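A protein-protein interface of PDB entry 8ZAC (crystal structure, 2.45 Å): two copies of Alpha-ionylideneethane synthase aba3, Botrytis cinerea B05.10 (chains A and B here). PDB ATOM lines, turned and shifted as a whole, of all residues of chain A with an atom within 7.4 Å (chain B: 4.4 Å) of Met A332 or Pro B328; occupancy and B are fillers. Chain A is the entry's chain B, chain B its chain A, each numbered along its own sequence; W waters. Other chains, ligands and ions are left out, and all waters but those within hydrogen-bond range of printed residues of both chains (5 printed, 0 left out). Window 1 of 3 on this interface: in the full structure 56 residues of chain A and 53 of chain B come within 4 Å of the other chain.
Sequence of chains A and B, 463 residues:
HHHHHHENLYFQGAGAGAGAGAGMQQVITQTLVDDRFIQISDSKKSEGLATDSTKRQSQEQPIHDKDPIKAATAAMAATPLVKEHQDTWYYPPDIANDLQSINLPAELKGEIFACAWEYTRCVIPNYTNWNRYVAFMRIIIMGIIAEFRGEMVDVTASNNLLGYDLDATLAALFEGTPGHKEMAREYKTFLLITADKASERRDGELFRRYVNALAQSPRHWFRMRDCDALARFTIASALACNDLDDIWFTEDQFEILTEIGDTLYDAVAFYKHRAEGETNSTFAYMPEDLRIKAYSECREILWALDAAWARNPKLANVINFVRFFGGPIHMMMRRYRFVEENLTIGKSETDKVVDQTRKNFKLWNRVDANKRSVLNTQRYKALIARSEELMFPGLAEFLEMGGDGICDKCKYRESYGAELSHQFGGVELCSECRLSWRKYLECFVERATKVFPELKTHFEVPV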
ATOM      1  N   GLU A 118     -32.877   9.633  24.678  1.00  0.00           N
ATOM      2  CA  GLU A 118     -32.082   8.711  23.844  1.00  0.00           C
ATOM      3  C   GLU A 118     -30.990   8.080  24.732  1.00  0.00           C
ATOM      4  O   GLU A 118     -30.806   6.820  24.656  1.00  0.00           O
ATOM      5  CB  GLU A 118     -31.521   9.412  22.616  1.00  0.00           C
ATOM      6  CG  GLU A 118     -32.570   9.847  21.618  1.00  0.00           C
ATOM      7  CD  GLU A 118     -32.038  10.330  20.288  1.00  0.00           C
ATOM      8  OE1 GLU A 118     -30.802  10.283  20.126  1.00  0.00           O
ATOM      9  OE2 GLU A 118     -32.860  10.735  19.408  1.00  0.00           O
ATOM     10  N   ARG A 121     -32.495   5.504  27.379  1.00  0.00           N
ATOM     11  CA  ARG A 121     -33.013   4.269  26.756  1.00  0.00           C
ATOM     12  C   ARG A 121     -31.844   3.425  26.276  1.00  0.00           C
ATOM     13  O   ARG A 121     -32.014   2.189  26.268  1.00  0.00           O
ATOM     14  CB  ARG A 121     -33.974   4.584  25.613  1.00  0.00           C
ATOM     15  CG  ARG A 121     -35.320   5.103  26.094  1.00  0.00           C
ATOM     16  CD  ARG A 121     -36.235   4.060  26.700  1.00  0.00           C
ATOM     17  NE  ARG A 121     -36.544   3.006  25.739  1.00  0.00           N
ATOM     18  CZ  ARG A 121     -36.165   1.736  25.847  1.00  0.00           C
ATOM     19  NH1 ARG A 121     -35.484   1.311  26.905  1.00  0.00           N
ATOM     20  NH2 ARG A 121     -36.452   0.890  24.872  1.00  0.00           N
ATOM     21  N   CYS A 122     -30.708   4.043  25.923  1.00  0.00           N
ATOM     22  CA  CYS A 122     -29.579   3.303  25.324  1.00  0.00           C
ATOM     23  C   CYS A 122     -28.843   2.615  26.471  1.00  0.00           C
ATOM     24  O   CYS A 122     -28.510   1.426  26.306  1.00  0.00           O
ATOM     25  CB  CYS A 122     -28.644   4.165  24.475  1.00  0.00           C
ATOM     26  SG  CYS A 122     -29.356   4.625  22.877  1.00  0.00           S
ATOM     27  N   VAL A 123     -28.589   3.322  27.575  1.00  0.00           N
ATOM     28  CA  VAL A 123     -27.654   2.802  28.606  1.00  0.00           C
ATOM     29  C   VAL A 123     -28.453   2.204  29.768  1.00  0.00           C
ATOM     30  O   VAL A 123     -27.837   1.457  30.534  1.00  0.00           O
ATOM     31  CB  VAL A 123     -26.595   3.825  29.061  1.00  0.00           C
ATOM     32  CG1 VAL A 123     -25.686   4.256  27.903  1.00  0.00           C
ATOM     33  CG2 VAL A 123     -27.189   5.005  29.806  1.00  0.00           C
ATOM     34  N   TYR A 295      -9.545  -2.423  24.454  1.00  0.00           N
ATOM     35  CA  TYR A 295     -10.936  -2.612  24.002  1.00  0.00           C
ATOM     36  C   TYR A 295     -11.202  -4.116  23.952  1.00  0.00           C
ATOM     37  O   TYR A 295     -12.280  -4.578  24.511  1.00  0.00           O
ATOM     38  CB  TYR A 295     -11.189  -1.940  22.652  1.00  0.00           C
ATOM     39  CG  TYR A 295     -12.618  -2.117  22.212  1.00  0.00           C
ATOM     40  CD1 TYR A 295     -13.017  -3.276  21.569  1.00  0.00           C
ATOM     41  CD2 TYR A 295     -13.592  -1.176  22.527  1.00  0.00           C
ATOM     42  CE1 TYR A 295     -14.344  -3.497  21.233  1.00  0.00           C
ATOM     43  CE2 TYR A 295     -14.918  -1.368  22.177  1.00  0.00           C
ATOM     44  CZ  TYR A 295     -15.288  -2.524  21.511  1.00  0.00           C
ATOM     45  OH  TYR A 295     -16.570  -2.734  21.129  1.00  0.00           O
ATOM     46  N   ARG A 323     -22.123  -2.080  28.467  1.00  0.00           N
ATOM     47  CA  ARG A 323     -21.964  -2.560  27.068  1.00  0.00           C
ATOM     48  C   ARG A 323     -22.385  -1.463  26.099  1.00  0.00           C
ATOM     49  O   ARG A 323     -21.632  -1.212  25.146  1.00  0.00           O
ATOM     50  CB  ARG A 323     -22.751  -3.850  26.851  1.00  0.00           C
ATOM     51  CG  ARG A 323     -22.695  -4.417  25.448  1.00  0.00           C
ATOM     52  CD  ARG A 323     -23.227  -5.839  25.426  1.00  0.00           C
ATOM     53  NE  ARG A 323     -22.204  -6.742  25.962  1.00  0.00           N
ATOM     54  CZ  ARG A 323     -22.423  -7.671  26.870  1.00  0.00           C
ATOM     55  NH1 ARG A 323     -23.641  -7.861  27.349  1.00  0.00           N
ATOM     56  NH2 ARG A 323     -21.416  -8.424  27.287  1.00  0.00           N
ATOM     57  N   PHE A 324     -23.545  -0.867  26.330  1.00  0.00           N
ATOM     58  CA  PHE A 324     -24.203   0.087  25.405  1.00  0.00           C
ATOM     59  C   PHE A 324     -23.514   1.456  25.501  1.00  0.00           C
ATOM     60  O   PHE A 324     -23.292   2.139  24.482  1.00  0.00           O
ATOM     61  CB  PHE A 324     -25.685   0.123  25.738  1.00  0.00           C
ATOM     62  CG  PHE A 324     -26.355  -1.198  25.517  1.00  0.00           C
ATOM     63  CD1 PHE A 324     -26.184  -1.883  24.333  1.00  0.00           C
ATOM     64  CD2 PHE A 324     -27.141  -1.769  26.492  1.00  0.00           C
ATOM     65  CE1 PHE A 324     -26.778  -3.117  24.129  1.00  0.00           C
ATOM     66  CE2 PHE A 324     -27.747  -2.999  26.283  1.00  0.00           C
ATOM     67  CZ  PHE A 324     -27.568  -3.665  25.102  1.00  0.00           C
ATOM     68  N   PHE A 325     -23.137   1.831  26.713  1.00  0.00           N
ATOM     69  CA  PHE A 325     -22.316   3.024  26.978  1.00  0.00           C
ATOM     70  C   PHE A 325     -21.015   2.881  26.210  1.00  0.00           C
ATOM     71  O   PHE A 325     -20.615   3.893  25.615  1.00  0.00           O
ATOM     72  CB  PHE A 325     -22.076   3.206  28.474  1.00  0.00           C
ATOM     73  CG  PHE A 325     -21.066   4.262  28.808  1.00  0.00           C
ATOM     74  CD1 PHE A 325     -21.444   5.603  28.901  1.00  0.00           C
ATOM     75  CD2 PHE A 325     -19.742   3.929  28.978  1.00  0.00           C
ATOM     76  CE1 PHE A 325     -20.503   6.590  29.164  1.00  0.00           C
ATOM     77  CE2 PHE A 325     -18.798   4.920  29.239  1.00  0.00           C
ATOM     78  CZ  PHE A 325     -19.179   6.245  29.334  1.00  0.00           C
ATOM     79  N   GLY A 327     -19.347   2.520  23.588  1.00  0.00           N
ATOM     80  CA  GLY A 327     -19.171   2.663  22.133  1.00  0.00           C
ATOM     81  C   GLY A 327     -20.489   2.664  21.361  1.00  0.00           C
ATOM     82  O   GLY A 327     -20.707   3.542  20.533  1.00  0.00           O
ATOM     83  N   PRO A 328     -21.380   1.671  21.556  1.00  0.00           N
ATOM     84  CA  PRO A 328     -22.619   1.587  20.769  1.00  0.00           C
ATOM     85  C   PRO A 328     -23.485   2.860  20.651  1.00  0.00           C
ATOM     86  O   PRO A 328     -24.180   3.033  19.649  1.00  0.00           O
ATOM     87  CB  PRO A 328     -23.384   0.480  21.514  1.00  0.00           C
ATOM     88  CG  PRO A 328     -22.283  -0.430  22.058  1.00  0.00           C
ATOM     89  CD  PRO A 328     -21.178   0.527  22.458  1.00  0.00           C
ATOM     90  N   ILE A 329     -23.481   3.723  21.664  1.00  0.00           N
ATOM     91  CA  ILE A 329     -24.335   4.941  21.676  1.00  0.00           C
ATOM     92  C   ILE A 329     -23.954   5.813  20.486  1.00  0.00           C
ATOM     93  O   ILE A 329     -24.825   6.557  20.046  1.00  0.00           O
ATOM     94  CB  ILE A 329     -24.305   5.700  23.022  1.00  0.00           C
ATOM     95  CG1 ILE A 329     -22.914   5.796  23.636  1.00  0.00           C
ATOM     96  CG2 ILE A 329     -25.261   5.066  24.006  1.00  0.00           C
ATOM     97  CD1 ILE A 329     -22.839   6.853  24.710  1.00  0.00           C
ATOM     98  N   HIS A 330     -22.727   5.693  19.966  1.00  0.00           N
ATOM     99  CA  HIS A 330     -22.236   6.421  18.764  1.00  0.00           C
ATOM    100  C   HIS A 330     -23.122   6.067  17.571  1.00  0.00           C
ATOM    101  O   HIS A 330     -23.400   6.975  16.771  1.00  0.00           O
ATOM    102  CB  HIS A 330     -20.771   6.121  18.472  1.00  0.00           C
ATOM    103  CG  HIS A 330     -19.828   6.772  19.429  1.00  0.00           C
ATOM    104  ND1 HIS A 330     -18.881   7.686  19.025  1.00  0.00           N
ATOM    105  CD2 HIS A 330     -19.694   6.657  20.771  1.00  0.00           C
ATOM    106  CE1 HIS A 330     -18.202   8.103  20.074  1.00  0.00           C
ATOM    107  NE2 HIS A 330     -18.688   7.491  21.160  1.00  0.00           N
ATOM    108  N   MET A 331     -23.611   4.825  17.496  1.00  0.00           N
ATOM    109  CA  MET A 331     -24.462   4.360  16.371  1.00  0.00           C
ATOM    110  C   MET A 331     -25.936   4.739  16.587  1.00  0.00           C
ATOM    111  O   MET A 331     -26.645   4.788  15.583  1.00  0.00           O
ATOM    112  CB  MET A 331     -24.356   2.848  16.178  1.00  0.00           C
ATOM    113  CG  MET A 331     -23.002   2.386  15.685  1.00  0.00           C
ATOM    114  SD  MET A 331     -22.969   0.602  15.311  1.00  0.00           S
ATOM    115  CE  MET A 331     -23.988   0.483  13.864  1.00  0.00           C
ATOM    116  N   MET A 332     -26.393   4.983  17.825  1.00  0.00           N
ATOM    117  CA  MET A 332     -27.847   4.911  18.190  1.00  0.00           C
ATOM    118  C   MET A 332     -28.409   6.297  18.532  1.00  0.00           C
ATOM    119  O   MET A 332     -29.635   6.486  18.358  1.00  0.00           O
ATOM    120  CB  MET A 332     -28.108   3.987  19.389  1.00  0.00           C
ATOM    121  CG  MET A 332     -27.448   2.627  19.276  1.00  0.00           C
ATOM    122  SD  MET A 332     -27.906   1.433  20.565  1.00  0.00           S
ATOM    123  CE  MET A 332     -26.856   1.913  21.937  1.00  0.00           C
ATOM    124  N   MET A 333     -27.581   7.214  19.038  1.00  0.00           N
ATOM    125  CA  MET A 333     -28.046   8.536  19.540  1.00  0.00           C
ATOM    126  C   MET A 333     -27.723   9.579  18.468  1.00  0.00           C
ATOM    127  O   MET A 333     -26.614   9.555  17.946  1.00  0.00           O
ATOM    128  CB  MET A 333     -27.338   8.932  20.839  1.00  0.00           C
ATOM    129  CG  MET A 333     -27.639   8.064  22.033  1.00  0.00           C
ATOM    130  SD  MET A 333     -26.726   8.618  23.456  1.00  0.00           S
ATOM    131  CE  MET A 333     -27.327  10.293  23.647  1.00  0.00           C
ATOM    132  N   ARG A 334     -28.640  10.501  18.213  1.00  0.00           N
ATOM    133  CA  ARG A 334     -28.492  11.557  17.163  1.00  0.00           C
ATOM    134  C   ARG A 334     -27.440  12.612  17.570  1.00  0.00           C
ATOM    135  O   ARG A 334     -26.874  13.209  16.657  1.00  0.00           O
ATOM    136  CB  ARG A 334     -29.906  12.007  16.783  1.00  0.00           C
ATOM    137  CG  ARG A 334     -30.708  10.774  16.406  1.00  0.00           C
ATOM    138  CD  ARG A 334     -32.026  10.997  15.764  1.00  0.00           C
ATOM    139  NE  ARG A 334     -33.024  11.217  16.780  1.00  0.00           N
ATOM    140  CZ  ARG A 334     -34.173  11.785  16.514  1.00  0.00           C
ATOM    141  NH1 ARG A 334     -35.054  11.963  17.478  1.00  0.00           N
ATOM    142  NH2 ARG A 334     -34.414  12.205  15.284  1.00  0.00           N
ATOM    143  N   ARG A 335     -27.099  12.709  18.855  1.00  0.00           N
ATOM    144  CA  ARG A 335     -26.051  13.587  19.438  1.00  0.00           C
ATOM    145  C   ARG A 335     -24.704  13.300  18.758  1.00  0.00           C
ATOM    146  O   ARG A 335     -23.906  14.260  18.584  1.00  0.00           O
ATOM    147  CB  ARG A 335     -25.937  13.356  20.955  1.00  0.00           C
ATOM    148  CG  ARG A 335     -25.370  14.532  21.740  1.00  0.00           C
ATOM    149  CD  ARG A 335     -23.987  14.309  22.328  1.00  0.00           C
ATOM    150  NE  ARG A 335     -23.655  15.351  23.298  1.00  0.00           N
ATOM    151  CZ  ARG A 335     -23.970  15.325  24.598  1.00  0.00           C
ATOM    152  NH1 ARG A 335     -24.629  14.300  25.135  1.00  0.00           N
ATOM    153  NH2 ARG A 335     -23.609  16.339  25.363  1.00  0.00           N
ATOM    154  N   TYR A 336     -24.443  12.030  18.434  1.00  0.00           N
ATOM    155  CA  TYR A 336     -23.192  11.561  17.778  1.00  0.00           C
ATOM    156  C   TYR A 336     -23.359  11.710  16.264  1.00  0.00           C
ATOM    157  O   TYR A 336     -24.461  12.085  15.828  1.00  0.00           O
ATOM    158  CB  TYR A 336     -22.852  10.147  18.259  1.00  0.00           C
ATOM    159  CG  TYR A 336     -22.526  10.113  19.726  1.00  0.00           C
ATOM    160  CD1 TYR A 336     -21.273  10.495  20.175  1.00  0.00           C
ATOM    161  CD2 TYR A 336     -23.484   9.773  20.672  1.00  0.00           C
ATOM    162  CE1 TYR A 336     -20.958  10.478  21.527  1.00  0.00           C
ATOM    163  CE2 TYR A 336     -23.190   9.746  22.023  1.00  0.00           C
ATOM    164  CZ  TYR A 336     -21.920  10.104  22.451  1.00  0.00           C
ATOM    165  OH  TYR A 336     -21.592  10.081  23.775  1.00  0.00           O
ATOM    166  N   PHE A 338     -22.550   9.458  13.587  1.00  0.00           N
ATOM    167  CA  PHE A 338     -22.595   8.247  12.734  1.00  0.00           C
ATOM    168  C   PHE A 338     -23.151   8.585  11.340  1.00  0.00           C
ATOM    169  O   PHE A 338     -22.528   8.219  10.298  1.00  0.00           O
ATOM    170  CB  PHE A 338     -23.468   7.181  13.374  1.00  0.00           C
ATOM    171  CG  PHE A 338     -23.390   5.823  12.736  1.00  0.00           C
ATOM    172  CD1 PHE A 338     -22.159   5.219  12.533  1.00  0.00           C
ATOM    173  CD2 PHE A 338     -24.546   5.126  12.395  1.00  0.00           C
ATOM    174  CE1 PHE A 338     -22.071   3.947  11.992  1.00  0.00           C
ATOM    175  CE2 PHE A 338     -24.445   3.844  11.872  1.00  0.00           C
ATOM    176  CZ  PHE A 338     -23.211   3.254  11.690  1.00  0.00           C
ATOM    177  N   ILE A 345     -17.661   4.597  11.856  1.00  0.00           N
ATOM    178  CA  ILE A 345     -17.006   4.962  13.135  1.00  0.00           C
ATOM    179  C   ILE A 345     -15.484   4.893  12.925  1.00  0.00           C
ATOM    180  O   ILE A 345     -14.983   3.948  12.297  1.00  0.00           O
ATOM    181  CB  ILE A 345     -17.558   4.074  14.277  1.00  0.00           C
ATOM    182  CG1 ILE A 345     -18.844   4.673  14.863  1.00  0.00           C
ATOM    183  CG2 ILE A 345     -16.543   3.848  15.379  1.00  0.00           C
ATOM    184  CD1 ILE A 345     -19.963   3.688  14.969  1.00  0.00           C
ATOM    185  N   ARG B 299     -34.050   5.120  12.053  1.00  0.00           N
ATOM    186  CA  ARG B 299     -33.587   5.396  13.438  1.00  0.00           C
ATOM    187  C   ARG B 299     -34.484   6.449  14.099  1.00  0.00           C
ATOM    188  O   ARG B 299     -34.751   6.309  15.326  1.00  0.00           O
ATOM    189  CB  ARG B 299     -32.130   5.851  13.472  1.00  0.00           C
ATOM    190  CG  ARG B 299     -31.615   6.102  14.880  1.00  0.00           C
ATOM    191  CD  ARG B 299     -30.144   6.466  14.908  1.00  0.00           C
ATOM    192  NE  ARG B 299     -29.834   7.792  14.379  1.00  0.00           N
ATOM    193  CZ  ARG B 299     -28.611   8.308  14.365  1.00  0.00           C
ATOM    194  NH1 ARG B 299     -27.586   7.622  14.850  1.00  0.00           N
ATOM    195  NH2 ARG B 299     -28.405   9.508  13.860  1.00  0.00           N
ATOM    196  N   TRP B 303     -37.143   5.937  17.293  1.00  0.00           N
ATOM    197  CA  TRP B 303     -37.125   6.851  18.477  1.00  0.00           C
ATOM    198  C   TRP B 303     -38.536   7.383  18.779  1.00  0.00           C
ATOM    199  O   TRP B 303     -38.884   7.452  19.977  1.00  0.00           O
ATOM    200  CB  TRP B 303     -36.131   8.021  18.325  1.00  0.00           C
ATOM    201  CG  TRP B 303     -34.737   7.632  18.668  1.00  0.00           C
ATOM    202  CD1 TRP B 303     -33.660   7.671  17.842  1.00  0.00           C
ATOM    203  CD2 TRP B 303     -34.279   7.061  19.898  1.00  0.00           C
ATOM    204  NE1 TRP B 303     -32.546   7.203  18.491  1.00  0.00           N
ATOM    205  CE2 TRP B 303     -32.895   6.818  19.750  1.00  0.00           C
ATOM    206  CE3 TRP B 303     -34.878   6.757  21.127  1.00  0.00           C
ATOM    207  CZ2 TRP B 303     -32.125   6.264  20.768  1.00  0.00           C
ATOM    208  CZ3 TRP B 303     -34.108   6.232  22.139  1.00  0.00           C
ATOM    209  CH2 TRP B 303     -32.756   5.968  21.952  1.00  0.00           C
ATOM    210  N   ARG B 323     -33.337  -1.886  17.873  1.00  0.00           N
ATOM    211  CA  ARG B 323     -32.219  -0.934  18.088  1.00  0.00           C
ATOM    212  C   ARG B 323     -30.861  -1.660  18.077  1.00  0.00           C
ATOM    213  O   ARG B 323     -29.920  -1.192  17.342  1.00  0.00           O
ATOM    214  CB  ARG B 323     -32.394  -0.204  19.414  1.00  0.00           C
ATOM    215  CG  ARG B 323     -31.340   0.869  19.673  1.00  0.00           C
ATOM    216  CD  ARG B 323     -31.762   1.901  20.716  1.00  0.00           C
ATOM    217  NE  ARG B 323     -32.908   2.624  20.175  1.00  0.00           N
ATOM    218  CZ  ARG B 323     -33.964   3.046  20.859  1.00  0.00           C
ATOM    219  NH1 ARG B 323     -34.070   2.834  22.162  1.00  0.00           N
ATOM    220  NH2 ARG B 323     -34.932   3.673  20.208  1.00  0.00           N
ATOM    221  N   PHE B 324     -30.735  -2.762  18.819  1.00  0.00           N
ATOM    222  CA  PHE B 324     -29.410  -3.372  19.102  1.00  0.00           C
ATOM    223  C   PHE B 324     -29.028  -4.257  17.926  1.00  0.00           C
ATOM    224  O   PHE B 324     -27.834  -4.275  17.561  1.00  0.00           O
ATOM    225  CB  PHE B 324     -29.381  -4.072  20.462  1.00  0.00           C
ATOM    226  CG  PHE B 324     -29.624  -3.137  21.623  1.00  0.00           C
ATOM    227  CD1 PHE B 324     -28.923  -1.944  21.736  1.00  0.00           C
ATOM    228  CD2 PHE B 324     -30.551  -3.443  22.604  1.00  0.00           C
ATOM    229  CE1 PHE B 324     -29.136  -1.091  22.810  1.00  0.00           C
ATOM    230  CE2 PHE B 324     -30.758  -2.587  23.676  1.00  0.00           C
ATOM    231  CZ  PHE B 324     -30.068  -1.407  23.769  1.00  0.00           C
ATOM    232  N   GLY B 326     -30.017  -3.520  14.807  1.00  0.00           N
ATOM    233  CA  GLY B 326     -29.831  -2.638  13.632  1.00  0.00           C
ATOM    234  C   GLY B 326     -28.494  -1.926  13.627  1.00  0.00           C
ATOM    235  O   GLY B 326     -28.498  -0.708  13.585  1.00  0.00           O
ATOM    236  N   GLY B 327     -27.388  -2.660  13.733  1.00  0.00           N
ATOM    237  CA  GLY B 327     -26.050  -2.069  13.651  1.00  0.00           C
ATOM    238  C   GLY B 327     -25.178  -2.375  14.854  1.00  0.00           C
ATOM    239  O   GLY B 327     -24.047  -2.841  14.674  1.00  0.00           O
ATOM    240  N   PRO B 328     -25.606  -2.015  16.089  1.00  0.00           N
ATOM    241  CA  PRO B 328     -24.724  -2.115  17.255  1.00  0.00           C
ATOM    242  C   PRO B 328     -24.055  -3.474  17.498  1.00  0.00           C
ATOM    243  O   PRO B 328     -22.988  -3.499  18.091  1.00  0.00           O
ATOM    244  CB  PRO B 328     -25.688  -1.779  18.417  1.00  0.00           C
ATOM    245  CG  PRO B 328     -26.648  -0.782  17.801  1.00  0.00           C
ATOM    246  CD  PRO B 328     -26.888  -1.365  16.420  1.00  0.00           C
ATOM    247  N   ILE B 329     -24.684  -4.582  17.095  1.00  0.00           N
ATOM    248  CA  ILE B 329     -24.080  -5.931  17.283  1.00  0.00           C
ATOM    249  C   ILE B 329     -22.701  -5.993  16.620  1.00  0.00           C
ATOM    250  O   ILE B 329     -21.878  -6.719  17.133  1.00  0.00           O
ATOM    251  CB  ILE B 329     -25.020  -7.079  16.873  1.00  0.00           C
ATOM    252  CG1 ILE B 329     -25.768  -6.814  15.566  1.00  0.00           C
ATOM    253  CG2 ILE B 329     -25.967  -7.384  18.029  1.00  0.00           C
ATOM    254  CD1 ILE B 329     -26.471  -8.041  15.031  1.00  0.00           C
ATOM    255  N   HIS B 330     -22.424  -5.210  15.587  1.00  0.00           N
ATOM    256  CA  HIS B 330     -21.109  -5.186  14.884  1.00  0.00           C
ATOM    257  C   HIS B 330     -19.983  -4.766  15.835  1.00  0.00           C
ATOM    258  O   HIS B 330     -18.859  -5.195  15.642  1.00  0.00           O
ATOM    259  CB  HIS B 330     -21.149  -4.251  13.676  1.00  0.00           C
ATOM    260  CG  HIS B 330     -21.840  -4.836  12.500  1.00  0.00           C
ATOM    261  ND1 HIS B 330     -21.163  -5.153  11.345  1.00  0.00           N
ATOM    262  CD2 HIS B 330     -23.128  -5.162  12.295  1.00  0.00           C
ATOM    263  CE1 HIS B 330     -22.011  -5.651  10.476  1.00  0.00           C
ATOM    264  NE2 HIS B 330     -23.223  -5.669  11.031  1.00  0.00           N
ATOM    265  N   MET B 331     -20.290  -3.936  16.820  1.00  0.00           N
ATOM    266  CA  MET B 331     -19.326  -3.447  17.816  1.00  0.00           C
ATOM    267  C   MET B 331     -19.211  -4.461  18.952  1.00  0.00           C
ATOM    268  O   MET B 331     -18.143  -4.531  19.536  1.00  0.00           O
ATOM    269  CB  MET B 331     -19.802  -2.126  18.392  1.00  0.00           C
ATOM    270  CG  MET B 331     -19.678  -0.921  17.467  1.00  0.00           C
ATOM    271  SD  MET B 331     -19.904   0.560  18.501  1.00  0.00           S
ATOM    272  CE  MET B 331     -18.956   1.794  17.623  1.00  0.00           C
ATOM    273  N   MET B 332     -20.270  -5.218  19.243  1.00  0.00           N
ATOM    274  CA  MET B 332     -20.490  -5.835  20.577  1.00  0.00           C
ATOM    275  C   MET B 332     -20.136  -7.329  20.572  1.00  0.00           C
ATOM    276  O   MET B 332     -19.791  -7.878  21.656  1.00  0.00           O
ATOM    277  CB  MET B 332     -21.944  -5.668  21.015  1.00  0.00           C
ATOM    278  CG  MET B 332     -22.292  -4.204  21.275  1.00  0.00           C
ATOM    279  SD  MET B 332     -23.894  -3.951  22.071  1.00  0.00           S
ATOM    280  CE  MET B 332     -25.020  -4.754  20.940  1.00  0.00           C
HETATM  281  O   HOH W   1     -31.265   4.110  17.841  1.00  0.00           O
HETATM  282  O   HOH W   2     -25.868  10.519  13.522  1.00  0.00           O
HETATM  283  O   HOH W   3     -25.149   8.624  16.131  1.00  0.00           O
HETATM  284  O   HOH W   4     -19.976  -6.296  23.952  1.00  0.00           O
HETATM  285  O   HOH W   5     -32.866   1.022  23.992  1.00  0.00           O
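Of the printed residues of chain B, Cys A122 touches Trp B303 (3.8 Å). Printed residues of chain B within 4 Å of Tyr A295: Met B331. Met A332 touches just these residues of chain B: Arg B299 (3.5 Å), Trp B303 (3.0 Å), Arg B323 (3.6 Å), Phe B324 (3.6 Å) and Pro B328 (3.8 Å). Printed residues of chain A within 4 Å of Arg B299: Met A331, Met A332, Met A333 and Arg A334. Of chain A, only Met A331 and Met A332 come within 4 Å of Pro B328. Of the printed residues of chain A, Met B331 touches Tyr A295 (2.9 Å), Gly A327 (3.6 Å), Pro A328 (3.6 Å) and Ile A345 (3.4 Å). The nearest printed residue of chain B that does not touch Met A332 is Met B332 (6.6 Å). The nearest residue of chain A that does not touch Pro B328 is Pro A328 (4.5 Å). The nearest printed residue of chain A that does not touch Phe B324 is Cys A122 (4.1 Å).
Water W5 lies within hydrogen-bond range of O of Arg A121 and NH1 of Arg B323. Water W2 lies within hydrogen-bond range of the guanidinium group (NH2) of Arg B299 (2.8 Å), the backbone carbonyl oxygen (O) of Tyr A336 (3.1 Å) and the backbone NH (N) of Phe A338 (3.5 Å). Water W4 bridges the backbone carbonyl oxygen (O) of Met B332 and the guanidinium group (NE) of Arg A323. Water W1 lies within hydrogen-bond range of O of Met A332, NE of Arg B323 and NE1 of Trp B303.
Arg A323 touches Met B332, and with the chains exchanged Met A332 touches Arg B323. Gly A327 touches Met B331, and with the chains exchanged Met A331 touches Gly B327. Pro A328 touches Met B331, and with the chains exchanged Met A331 touches Pro B328. Pro A328 touches Met B332, and with the chains exchanged Met A332 touches Pro B328. Positions printed for both chains: 323, 324, 327, 328, 329, 330, 331 and 332. Of the 23 pairs that touch across the chains among the printed residues, 11 have their exchanged pair printed and touching as well.
The backbone carbonyl oxygen of Met A331 sits at hydrogen-bond distance from the guanidinium group of Arg B299 (3.1 Å). NE1 of Trp B303 is in hydrogen-bond range of O of Met A332 (3.0 Å). The backbone carbonyl oxygen of Met B331 sits at hydrogen-bond distance from the side-chain hydroxyl of Tyr A295. The side-chain sulfur (SD) of Met B331 lies close to the backbone carbonyl oxygen (O) of Gly A327, at 3.7 Å. The backbone nitrogen (N) of Pro A328 lies close to the side-chain sulfur (SD) of Met B331 (3.6 Å). The side-chain sulfur of Met A331 sits close to the backbone carbonyl oxygen of Gly B327, 3.7 Å away. The side-chain sulfur of Met A331 lies close to the backbone nitrogen of Pro B328, 3.8 Å away.
Among the printed residues, pairs that only touch across the chains: Phe A324 with Phe B324 (3.4 Å), Glu A118 with Trp B303 (3.4 Å), Ile A345 with Met B331 (3.4 Å), Met A332 with Arg B299 (3.5 Å), Met A332 with Arg B323 (3.6 Å), Met A332 with Phe B324 (3.6 Å), Arg A323 with Met B332 (3.6 Å), Phe A324 with Met B332 (3.6 Å), Arg A334 with Arg B299 (3.7 Å), Arg A334 with Trp B303 (3.8 Å), Met A332 with Pro B328 (3.8 Å), Cys A122 with Trp B303 (3.8 Å), Met A333 with Arg B299 (3.8 Å), Arg A121 with Trp B303 (3.8 Å), Pro A328 with Met B332 (3.9 Å) and Arg A121 with Arg B323 (3.9 Å).
O of Phe B324 lies within hydrogen-bond range of N of Ile B329. O of Glu A118 is in hydrogen-bond range of SG of Cys A122 (3.2 Å). NE of Arg A334 is in salt-bridge range of OE2 of Glu A118. O of Phe A324 sits at hydrogen-bond distance from N of Ile A329.
Of the 11 printed residues of chain B, 8 touch a printed residue of chain A. Hydrophobic or aromatic side chains of chain B that line the printed part of chain A: Trp B303, Phe B324, Pro B328, Met B331 and Met B332. Hydrophobic or aromatic side chains of chain A that line the printed part of chain B: Tyr A295, Phe A324, Pro A328, Met A331, Met A332 and Ile A345.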
